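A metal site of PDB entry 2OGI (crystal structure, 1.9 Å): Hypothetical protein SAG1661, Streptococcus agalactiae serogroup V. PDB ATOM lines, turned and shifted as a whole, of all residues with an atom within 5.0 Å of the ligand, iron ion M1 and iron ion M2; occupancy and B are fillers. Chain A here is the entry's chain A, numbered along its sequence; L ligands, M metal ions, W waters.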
ATOM      1  N   HIS A  30      17.181  20.140  16.517  1.00  0.00           N
ATOM      2  CA  HIS A  30      17.839  18.912  16.865  1.00  0.00           C
ATOM      3  C   HIS A  30      18.505  18.320  15.653  1.00  0.00           C
ATOM      4  O   HIS A  30      19.652  17.886  15.694  1.00  0.00           O
ATOM      5  CB  HIS A  30      16.853  17.940  17.460  1.00  0.00           C
ATOM      6  CG  HIS A  30      17.298  16.511  17.416  1.00  0.00           C
ATOM      7  ND1 HIS A  30      18.307  16.048  18.211  1.00  0.00           N
ATOM      8  CD2 HIS A  30      16.856  15.461  16.695  1.00  0.00           C
ATOM      9  CE1 HIS A  30      18.478  14.745  17.983  1.00  0.00           C
ATOM     10  NE2 HIS A  30      17.573  14.361  17.095  1.00  0.00           N
ATOM     11  N   VAL A  34      22.330  17.453  15.049  1.00  0.00           N
ATOM     12  CA  VAL A  34      22.832  16.159  14.641  1.00  0.00           C
ATOM     13  C   VAL A  34      23.665  16.217  13.364  1.00  0.00           C
ATOM     14  O   VAL A  34      24.680  15.545  13.245  1.00  0.00           O
ATOM     15  CB  VAL A  34      21.680  15.119  14.492  1.00  0.00           C
ATOM     16  CG1 VAL A  34      22.251  13.753  14.054  1.00  0.00           C
ATOM     17  CG2 VAL A  34      20.973  14.949  15.812  1.00  0.00           C
ATOM     18  N   HIS A  59      17.643  11.899   9.396  1.00  0.00           N
ATOM     19  CA  HIS A  59      17.427  10.701  10.251  1.00  0.00           C
ATOM     20  C   HIS A  59      16.061  10.676  10.930  1.00  0.00           C
ATOM     21  O   HIS A  59      15.468   9.633  11.078  1.00  0.00           O
ATOM     22  CB  HIS A  59      18.586  10.516  11.248  1.00  0.00           C
ATOM     23  CG  HIS A  59      18.482  11.367  12.440  1.00  0.00           C
ATOM     24  ND1 HIS A  59      18.736  12.718  12.422  1.00  0.00           N
ATOM     25  CD2 HIS A  59      18.055  11.088  13.683  1.00  0.00           C
ATOM     26  CE1 HIS A  59      18.489  13.225  13.617  1.00  0.00           C
ATOM     27  NE2 HIS A  59      18.048  12.260  14.401  1.00  0.00           N
ATOM     28  N   ASP A  60      15.574  11.846  11.311  1.00  0.00           N
ATOM     29  CA  ASP A  60      14.285  12.043  11.963  1.00  0.00           C
ATOM     30  C   ASP A  60      13.248  12.632  11.036  1.00  0.00           C
ATOM     31  O   ASP A  60      12.352  13.256  11.480  1.00  0.00           O
ATOM     32  CB  ASP A  60      14.482  12.949  13.181  1.00  0.00           C
ATOM     33  CG  ASP A  60      14.796  12.135  14.467  1.00  0.00           C
ATOM     34  OD1 ASP A  60      14.635  10.874  14.461  1.00  0.00           O
ATOM     35  OD2 ASP A  60      15.230  12.754  15.467  1.00  0.00           O
ATOM     36  N   LYS A  63       9.800  11.589  12.172  1.00  0.00           N
ATOM     37  CA  LYS A  63       9.597  11.563  13.603  1.00  0.00           C
ATOM     38  C   LYS A  63       8.168  11.929  14.015  1.00  0.00           C
ATOM     39  O   LYS A  63       7.660  11.392  14.973  1.00  0.00           O
ATOM     40  CB  LYS A  63      10.587  12.511  14.274  1.00  0.00           C
ATOM     41  CG  LYS A  63      10.583  12.581  15.795  1.00  0.00           C
ATOM     42  CD  LYS A  63      10.901  11.284  16.524  1.00  0.00           C
ATOM     43  CE  LYS A  63      11.221  11.621  17.966  1.00  0.00           C
ATOM     44  NZ  LYS A  63      11.411  10.485  18.879  1.00  0.00           N
ATOM     45  N   TRP A  86       4.535  -2.087  18.183  1.00  0.00           N
ATOM     46  CA  TRP A  86       5.434  -1.139  18.766  1.00  0.00           C
ATOM     47  C   TRP A  86       4.841   0.251  18.545  1.00  0.00           C
ATOM     48  O   TRP A  86       3.624   0.446  18.625  1.00  0.00           O
ATOM     49  CB  TRP A  86       6.858  -1.324  18.248  1.00  0.00           C
ATOM     50  CG  TRP A  86       7.416  -2.651  18.627  1.00  0.00           C
ATOM     51  CD1 TRP A  86       7.243  -3.806  17.973  1.00  0.00           C
ATOM     52  CD2 TRP A  86       8.195  -2.960  19.782  1.00  0.00           C
ATOM     53  NE1 TRP A  86       7.885  -4.837  18.623  1.00  0.00           N
ATOM     54  CE2 TRP A  86       8.485  -4.338  19.736  1.00  0.00           C
ATOM     55  CE3 TRP A  86       8.736  -2.192  20.826  1.00  0.00           C
ATOM     56  CZ2 TRP A  86       9.246  -4.986  20.724  1.00  0.00           C
ATOM     57  CZ3 TRP A  86       9.498  -2.844  21.823  1.00  0.00           C
ATOM     58  CH2 TRP A  86       9.732  -4.222  21.763  1.00  0.00           C
ATOM     59  N   ASN A  89       8.650   5.280  18.378  1.00  0.00           N
ATOM     60  CA  ASN A  89      10.061   5.227  18.719  1.00  0.00           C
ATOM     61  C   ASN A  89      10.758   4.262  17.778  1.00  0.00           C
ATOM     62  O   ASN A  89      11.866   4.479  17.254  1.00  0.00           O
ATOM     63  CB  ASN A  89      10.287   4.737  20.170  1.00  0.00           C
ATOM     64  CG  ASN A  89       9.996   5.777  21.211  1.00  0.00           C
ATOM     65  OD1 ASN A  89       9.742   6.953  20.903  1.00  0.00           O
ATOM     66  ND2 ASN A  89       9.978   5.337  22.478  1.00  0.00           N
ATOM     67  N   ILE A  90      10.082   3.158  17.533  1.00  0.00           N
ATOM     68  CA  ILE A  90      10.638   2.105  16.706  1.00  0.00           C
ATOM     69  C   ILE A  90      10.376   2.416  15.239  1.00  0.00           C
ATOM     70  O   ILE A  90      11.209   2.155  14.386  1.00  0.00           O
ATOM     71  CB  ILE A  90       9.990   0.726  17.091  1.00  0.00           C
ATOM     72  CG1 ILE A  90      10.391   0.283  18.503  1.00  0.00           C
ATOM     73  CG2 ILE A  90      10.328  -0.352  16.112  1.00  0.00           C
ATOM     74  CD1 ILE A  90      11.756   0.613  18.884  1.00  0.00           C
ATOM     75  N   HIS A  92       9.794   5.313  13.514  1.00  0.00           N
ATOM     76  CA  HIS A  92      10.154   6.506  12.723  1.00  0.00           C
ATOM     77  C   HIS A  92      11.411   6.364  11.922  1.00  0.00           C
ATOM     78  O   HIS A  92      11.518   7.074  10.911  1.00  0.00           O
ATOM     79  CB  HIS A  92      10.115   7.811  13.558  1.00  0.00           C
ATOM     80  CG  HIS A  92      11.265   7.963  14.516  1.00  0.00           C
ATOM     81  ND1 HIS A  92      11.281   7.330  15.735  1.00  0.00           N
ATOM     82  CD2 HIS A  92      12.457   8.608  14.396  1.00  0.00           C
ATOM     83  CE1 HIS A  92      12.429   7.613  16.361  1.00  0.00           C
ATOM     84  NE2 HIS A  92      13.157   8.376  15.563  1.00  0.00           N
ATOM     85  N   HIS A 118      18.858   4.041  13.266  1.00  0.00           N
ATOM     86  CA  HIS A 118      19.392   5.098  14.126  1.00  0.00           C
ATOM     87  C   HIS A 118      18.929   5.016  15.570  1.00  0.00           C
ATOM     88  O   HIS A 118      19.645   5.476  16.430  1.00  0.00           O
ATOM     89  CB  HIS A 118      19.146   6.513  13.557  1.00  0.00           C
ATOM     90  CG  HIS A 118      17.805   7.100  13.870  1.00  0.00           C
ATOM     91  ND1 HIS A 118      16.742   7.017  12.995  1.00  0.00           N
ATOM     92  CD2 HIS A 118      17.381   7.912  14.874  1.00  0.00           C
ATOM     93  CE1 HIS A 118      15.718   7.695  13.480  1.00  0.00           C
ATOM     94  NE2 HIS A 118      16.073   8.255  14.611  1.00  0.00           N
ATOM     95  N   THR A 119      17.775   4.429  15.844  1.00  0.00           N
ATOM     96  CA  THR A 119      17.234   4.388  17.196  1.00  0.00           C
ATOM     97  C   THR A 119      17.732   3.141  17.923  1.00  0.00           C
ATOM     98  O   THR A 119      18.151   3.196  19.046  1.00  0.00           O
ATOM     99  CB  THR A 119      15.672   4.419  17.184  1.00  0.00           C
ATOM    100  OG1 THR A 119      15.225   5.449  16.301  1.00  0.00           O
ATOM    101  CG2 THR A 119      15.098   4.585  18.603  1.00  0.00           C
ATOM    102  N   VAL A 120      17.764   1.995  17.251  1.00  0.00           N
ATOM    103  CA  VAL A 120      18.012   0.720  17.900  1.00  0.00           C
ATOM    104  C   VAL A 120      19.380   0.094  17.629  1.00  0.00           C
ATOM    105  O   VAL A 120      19.826  -0.772  18.373  1.00  0.00           O
ATOM    106  CB  VAL A 120      16.903  -0.273  17.502  1.00  0.00           C
ATOM    107  CG1 VAL A 120      15.598   0.259  18.011  1.00  0.00           C
ATOM    108  CG2 VAL A 120      16.795  -0.448  16.047  1.00  0.00           C
ATOM    109  N   ASP A 136      23.280  11.598  17.093  1.00  0.00           N
ATOM    110  CA  ASP A 136      21.902  11.813  17.573  1.00  0.00           C
ATOM    111  C   ASP A 136      21.816  12.034  19.078  1.00  0.00           C
ATOM    112  O   ASP A 136      20.982  12.803  19.570  1.00  0.00           O
ATOM    113  CB  ASP A 136      21.064  10.582  17.179  1.00  0.00           C
ATOM    114  CG  ASP A 136      19.576  10.794  17.397  1.00  0.00           C
ATOM    115  OD1 ASP A 136      19.101  11.957  17.236  1.00  0.00           O
ATOM    116  OD2 ASP A 136      18.908   9.819  17.795  1.00  0.00           O
ATOM    117  N   ARG A 142      21.223  18.677  23.118  1.00  0.00           N
ATOM    118  CA  ARG A 142      20.896  17.657  24.130  1.00  0.00           C
ATOM    119  C   ARG A 142      21.468  18.014  25.504  1.00  0.00           C
ATOM    120  O   ARG A 142      22.574  18.512  25.596  1.00  0.00           O
ATOM    121  CB  ARG A 142      21.432  16.271  23.769  1.00  0.00           C
ATOM    122  CG  ARG A 142      20.926  15.647  22.487  1.00  0.00           C
ATOM    123  CD  ARG A 142      19.520  15.120  22.594  1.00  0.00           C
ATOM    124  NE  ARG A 142      19.397  13.917  21.777  1.00  0.00           N
ATOM    125  CZ  ARG A 142      18.279  13.483  21.199  1.00  0.00           C
ATOM    126  NH1 ARG A 142      17.146  14.161  21.319  1.00  0.00           N
ATOM    127  NH2 ARG A 142      18.296  12.360  20.461  1.00  0.00           N
ATOM    128  N   THR A 169      20.567   3.611  27.424  1.00  0.00           N
ATOM    129  CA  THR A 169      19.216   3.575  26.929  1.00  0.00           C
ATOM    130  C   THR A 169      18.518   2.318  27.509  1.00  0.00           C
ATOM    131  O   THR A 169      17.395   2.370  27.886  1.00  0.00           O
ATOM    132  CB  THR A 169      19.209   3.550  25.390  1.00  0.00           C
ATOM    133  OG1 THR A 169      19.775   4.792  24.906  1.00  0.00           O
ATOM    134  CG2 THR A 169      17.849   3.296  24.841  1.00  0.00           C
ATOM    135  N   PHE A 172      17.674   2.995  31.061  1.00  0.00           N
ATOM    136  CA  PHE A 172      16.581   3.981  31.151  1.00  0.00           C
ATOM    137  C   PHE A 172      15.200   3.332  30.916  1.00  0.00           C
ATOM    138  O   PHE A 172      14.239   3.586  31.637  1.00  0.00           O
ATOM    139  CB  PHE A 172      16.843   5.098  30.136  1.00  0.00           C
ATOM    140  CG  PHE A 172      15.669   5.984  29.892  1.00  0.00           C
ATOM    141  CD1 PHE A 172      15.334   6.978  30.775  1.00  0.00           C
ATOM    142  CD2 PHE A 172      14.850   5.793  28.784  1.00  0.00           C
ATOM    143  CE1 PHE A 172      14.244   7.786  30.565  1.00  0.00           C
ATOM    144  CE2 PHE A 172      13.754   6.591  28.582  1.00  0.00           C
ATOM    145  CZ  PHE A 172      13.464   7.585  29.469  1.00  0.00           C
ATOM    146  N   LEU A 173      15.116   2.507  29.889  1.00  0.00           N
ATOM    147  CA  LEU A 173      13.877   1.846  29.506  1.00  0.00           C
ATOM    148  C   LEU A 173      13.445   0.870  30.596  1.00  0.00           C
ATOM    149  O   LEU A 173      12.279   0.767  30.916  1.00  0.00           O
ATOM    150  CB  LEU A 173      14.103   1.078  28.189  1.00  0.00           C
ATOM    151  CG  LEU A 173      14.301   1.925  26.902  1.00  0.00           C
ATOM    152  CD1 LEU A 173      14.686   1.015  25.744  1.00  0.00           C
ATOM    153  CD2 LEU A 173      13.056   2.710  26.578  1.00  0.00           C
ATOM    154  N   GLN A 178       9.505  -0.154  30.268  1.00  0.00           N
ATOM    155  CA  GLN A 178       9.057   0.035  28.881  1.00  0.00           C
ATOM    156  C   GLN A 178       9.657  -1.028  28.029  1.00  0.00           C
ATOM    157  O   GLN A 178      10.770  -1.475  28.278  1.00  0.00           O
ATOM    158  CB  GLN A 178       9.549   1.369  28.312  1.00  0.00           C
ATOM    159  CG  GLN A 178       9.041   2.590  29.040  1.00  0.00           C
ATOM    160  CD  GLN A 178       7.563   2.687  28.992  1.00  0.00           C
ATOM    161  OE1 GLN A 178       6.960   2.576  27.916  1.00  0.00           O
ATOM    162  NE2 GLN A 178       6.939   2.885  30.158  1.00  0.00           N
ATOM    163  N   PRO A 179       8.924  -1.432  26.994  1.00  0.00           N
ATOM    164  CA  PRO A 179       9.492  -2.539  26.216  1.00  0.00           C
ATOM    165  C   PRO A 179      10.763  -2.161  25.534  1.00  0.00           C
ATOM    166  O   PRO A 179      10.968  -0.990  25.189  1.00  0.00           O
ATOM    167  CB  PRO A 179       8.372  -2.924  25.224  1.00  0.00           C
ATOM    168  CG  PRO A 179       7.461  -1.781  25.198  1.00  0.00           C
ATOM    169  CD  PRO A 179       7.625  -0.974  26.469  1.00  0.00           C
ATOM    170  N   ILE A 180      11.614  -3.172  25.390  1.00  0.00           N
ATOM    171  CA  ILE A 180      12.906  -3.035  24.858  1.00  0.00           C
ATOM    172  C   ILE A 180      12.916  -3.861  23.580  1.00  0.00           C
ATOM    173  O   ILE A 180      12.700  -5.052  23.601  1.00  0.00           O
ATOM    174  CB  ILE A 180      13.985  -3.535  25.875  1.00  0.00           C
ATOM    175  CG1 ILE A 180      14.053  -2.602  27.072  1.00  0.00           C
ATOM    176  CG2 ILE A 180      15.341  -3.722  25.194  1.00  0.00           C
ATOM    177  CD1 ILE A 180      14.826  -3.173  28.242  1.00  0.00           C
ATOM    178  N   TYR A 181      13.126  -3.163  22.463  1.00  0.00           N
ATOM    179  CA  TYR A 181      13.163  -3.762  21.159  1.00  0.00           C
ATOM    180  C   TYR A 181      14.292  -4.699  21.114  1.00  0.00           C
ATOM    181  O   TYR A 181      15.351  -4.405  21.598  1.00  0.00           O
ATOM    182  CB  TYR A 181      13.275  -2.717  20.025  1.00  0.00           C
ATOM    183  CG  TYR A 181      12.908  -3.207  18.620  1.00  0.00           C
ATOM    184  CD1 TYR A 181      11.600  -3.599  18.322  1.00  0.00           C
ATOM    185  CD2 TYR A 181      13.860  -3.265  17.605  1.00  0.00           C
ATOM    186  CE1 TYR A 181      11.242  -4.017  17.061  1.00  0.00           C
ATOM    187  CE2 TYR A 181      13.510  -3.671  16.316  1.00  0.00           C
ATOM    188  CZ  TYR A 181      12.205  -4.039  16.065  1.00  0.00           C
ATOM    189  OH  TYR A 181      11.822  -4.457  14.821  1.00  0.00           O
ATOM    190  N   THR A 184      17.753  -3.673  20.035  1.00  0.00           N
ATOM    191  CA  THR A 184      18.426  -2.856  21.014  1.00  0.00           C
ATOM    192  C   THR A 184      19.376  -3.707  21.877  1.00  0.00           C
ATOM    193  O   THR A 184      20.472  -3.286  22.171  1.00  0.00           O
ATOM    194  CB  THR A 184      17.402  -2.105  21.855  1.00  0.00           C
ATOM    195  OG1 THR A 184      16.732  -1.252  20.957  1.00  0.00           O
ATOM    196  CG2 THR A 184      18.035  -1.252  22.966  1.00  0.00           C
HETATM  197  P1  LIG L   1      15.090  11.028  18.873  1.00  0.00           P
HETATM  198  O1  LIG L   1      14.246  11.407  20.065  1.00  0.00           O
HETATM  199  O2  LIG L   1      14.155  10.597  17.742  1.00  0.00           O
HETATM  200  O3  LIG L   1      16.074  12.140  18.475  1.00  0.00           O
HETATM  201  O4  LIG L   1      16.050   9.808  19.418  1.00  0.00           O
HETATM  202  P2  LIG L   1      15.959   8.234  19.012  1.00  0.00           P
HETATM  203  O5  LIG L   1      15.437   7.870  17.637  1.00  0.00           O
HETATM  204  O6  LIG L   1      17.298   7.578  19.300  1.00  0.00           O
HETATM  205  O7  LIG L   1      14.984   7.540  20.137  1.00  0.00           O
HETATM  206  C1  LIG L   1      13.698   8.017  20.483  1.00  0.00           C
HETATM  207  C2  LIG L   1      13.183   7.222  21.691  1.00  0.00           C
HETATM  208  O8  LIG L   1      13.196   5.837  21.351  1.00  0.00           O
HETATM  209  C3  LIG L   1      13.957   7.378  23.008  1.00  0.00           C
HETATM  210  O9  LIG L   1      13.054   7.707  24.076  1.00  0.00           O
HETATM  211  C4  LIG L   1      14.558   6.019  23.291  1.00  0.00           C
HETATM  212  O10 LIG L   1      14.565   5.688  24.685  1.00  0.00           O
HETATM  213  C5  LIG L   1      13.542   5.155  22.555  1.00  0.00           C
HETATM  214  N1  LIG L   1      14.074   3.797  22.350  1.00  0.00           N
HETATM  215  C6  LIG L   1      15.291   3.453  21.964  1.00  0.00           C
HETATM  216  N2  LIG L   1      15.400   2.093  21.902  1.00  0.00           N
HETATM  217  C7  LIG L   1      14.198   1.597  22.318  1.00  0.00           C
HETATM  218  C8  LIG L   1      13.634   0.265  22.575  1.00  0.00           C
HETATM  219  O11 LIG L   1      14.393  -0.705  22.342  1.00  0.00           O
HETATM  220  N3  LIG L   1      12.335   0.181  23.022  1.00  0.00           N
HETATM  221  C9  LIG L   1      11.558   1.304  23.275  1.00  0.00           C
HETATM  222  N4  LIG L   1      10.259   1.213  23.753  1.00  0.00           N
HETATM  223  N5  LIG L   1      12.052   2.563  23.058  1.00  0.00           N
HETATM  224  C10 LIG L   1      13.317   2.732  22.596  1.00  0.00           C
HETATM  225 FE    FE M   1      17.107  12.275  16.473  1.00  0.00          FE
HETATM  226 FE    FE M   2      15.036   9.469  16.069  1.00  0.00          FE
HETATM  227  O   HOH W   1      20.248   6.834  18.604  1.00  0.00           O
HETATM  228  O   HOH W   2      16.820  10.337  16.510  1.00  0.00           O
HETATM  229  O   HOH W   3      17.931   1.940  21.430  1.00  0.00           O
HETATM  230  O   HOH W   4      11.142   5.995  26.029  1.00  0.00           O
HETATM  231  O   HOH W   5       9.257   3.578  25.396  1.00  0.00           O
HETATM  232  O   HOH W   6      19.454   9.118  20.887  1.00  0.00           O
HETATM  233  O   HOH W   7      11.514  10.949  21.899  1.00  0.00           O
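Of the 22 residues printed, 3 come within 4 Å of iron ion M2.
Thr 169 touches the ligand (CG2 to C6, 3.9 Å).
CD1 of Leu 173 touches C8 of the ligand, at 3.4 Å.
Ile 180 touches the ligand.
Hydrophobic or aromatic side chains within 4 Å of the ligand: His 30, His 92, His 118, Leu 173 and Tyr 181.
Within 4 Å of the ligand: His 30, Asp 60, Lys 63, Asn 89, His 92, His 118, Thr 119, Asp 136, Arg 142, Thr 169, Leu 173, Pro 179, Ile 180, Tyr 181 and Thr 184.
The nearest printed residue that does not touch the ligand is Phe 172 (4.1 Å).
OD2 of Asp 136 is in salt-bridge range of NH2 of Arg 142 (3.7 Å).
O of His 59 sits close to ND1 of His 118, 3.5 Å away.
NE2 of His 118 sits close to OG1 of Thr 119.
A ring nitrogen (ND1) of His 92 is in hydrogen-bond range of the backbone carbonyl oxygen of Asn 89 (3.3 Å).
The backbone carbonyl oxygen of Leu 173 is in hydrogen-bond range of the backbone NH of Gln 178 (3.0 Å).
A nitrogen (N4) of the ligand sits at hydrogen-bond distance from the backbone carbonyl oxygen (O) of Pro 179 (2.7 Å).
N of Tyr 181 is in hydrogen-bond range of O11 of the ligand, 2.8 Å away.
OG1 of Thr 119 lies close to O5 of the ligand, 2.8 Å away.
The side-chain hydroxyl (OG1) of Thr 184 is in hydrogen-bond range of an oxygen (O11) of the ligand, at 2.8 Å.
NZ of Lys 63 lies within salt-bridge range of O1 of the ligand, at 3.2 Å.
An oxygen (O3) of the ligand lies close to the guanidinium group (NH2) of Arg 142, 3.0 Å away.
The side-chain amide nitrogen of Asn 89 lies close to an oxygen (O8) of the ligand, 3.4 Å away.
Water W2 bridges OD2 of Asp 136 (2.5 Å) and O4 of the ligand (3.1 Å).
Water W3 lies within hydrogen-bond range of a nitrogen (N2) of the ligand (2.6 Å), the backbone carbonyl oxygen (O) of Thr 119 (2.7 Å) and the side-chain hydroxyl (OG1) of Thr 184 (3.4 Å).
Water W5 bridges N4 of the ligand and ND2 of Asn 89.
Water W6 lies within hydrogen-bond range of an oxygen (O6) of the ligand (3.1 Å), the side-chain carboxylate (OD2) of Asp 136 (3.2 Å) and the guanidinium group (NH2) of Arg 142 (3.5 Å).
Water W1 lies within hydrogen-bond range of O of His 118 (2.6 Å), O6 of the ligand (3.1 Å) and OD2 of Asp 136 (3.4 Å).
Water W7 bridges NZ of Lys 63 (3.1 Å) and O1 of the ligand (3.3 Å).
Iron ion M1 is bound by water W2 (2.0 Å), the side-chain carboxylate (OD1) of Asp 136 (2.2 Å), the side-chain carboxylate (OD2) of Asp 60 (2.2 Å), a ring nitrogen (NE2) of His 30 (2.2 Å), an oxygen (O3) of the ligand (2.3 Å) and a ring nitrogen (NE2) of His 59 (2.3 Å).
Water W2 is bound to iron ion M2, 2.0 Å away.
Iron ion M2 is bound by a ring nitrogen (NE2) of His 118 (2.2 Å).
The side-chain carboxylate (OD1) of Asp 60 is bound to iron ion M2 (2.2 Å).
Iron ion M2 is bound by O2 of the ligand, at 2.2 Å.
Iron ion M2 is bound by NE2 of His 92.
O5 of the ligand binds iron ion M2 (2.3 Å).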
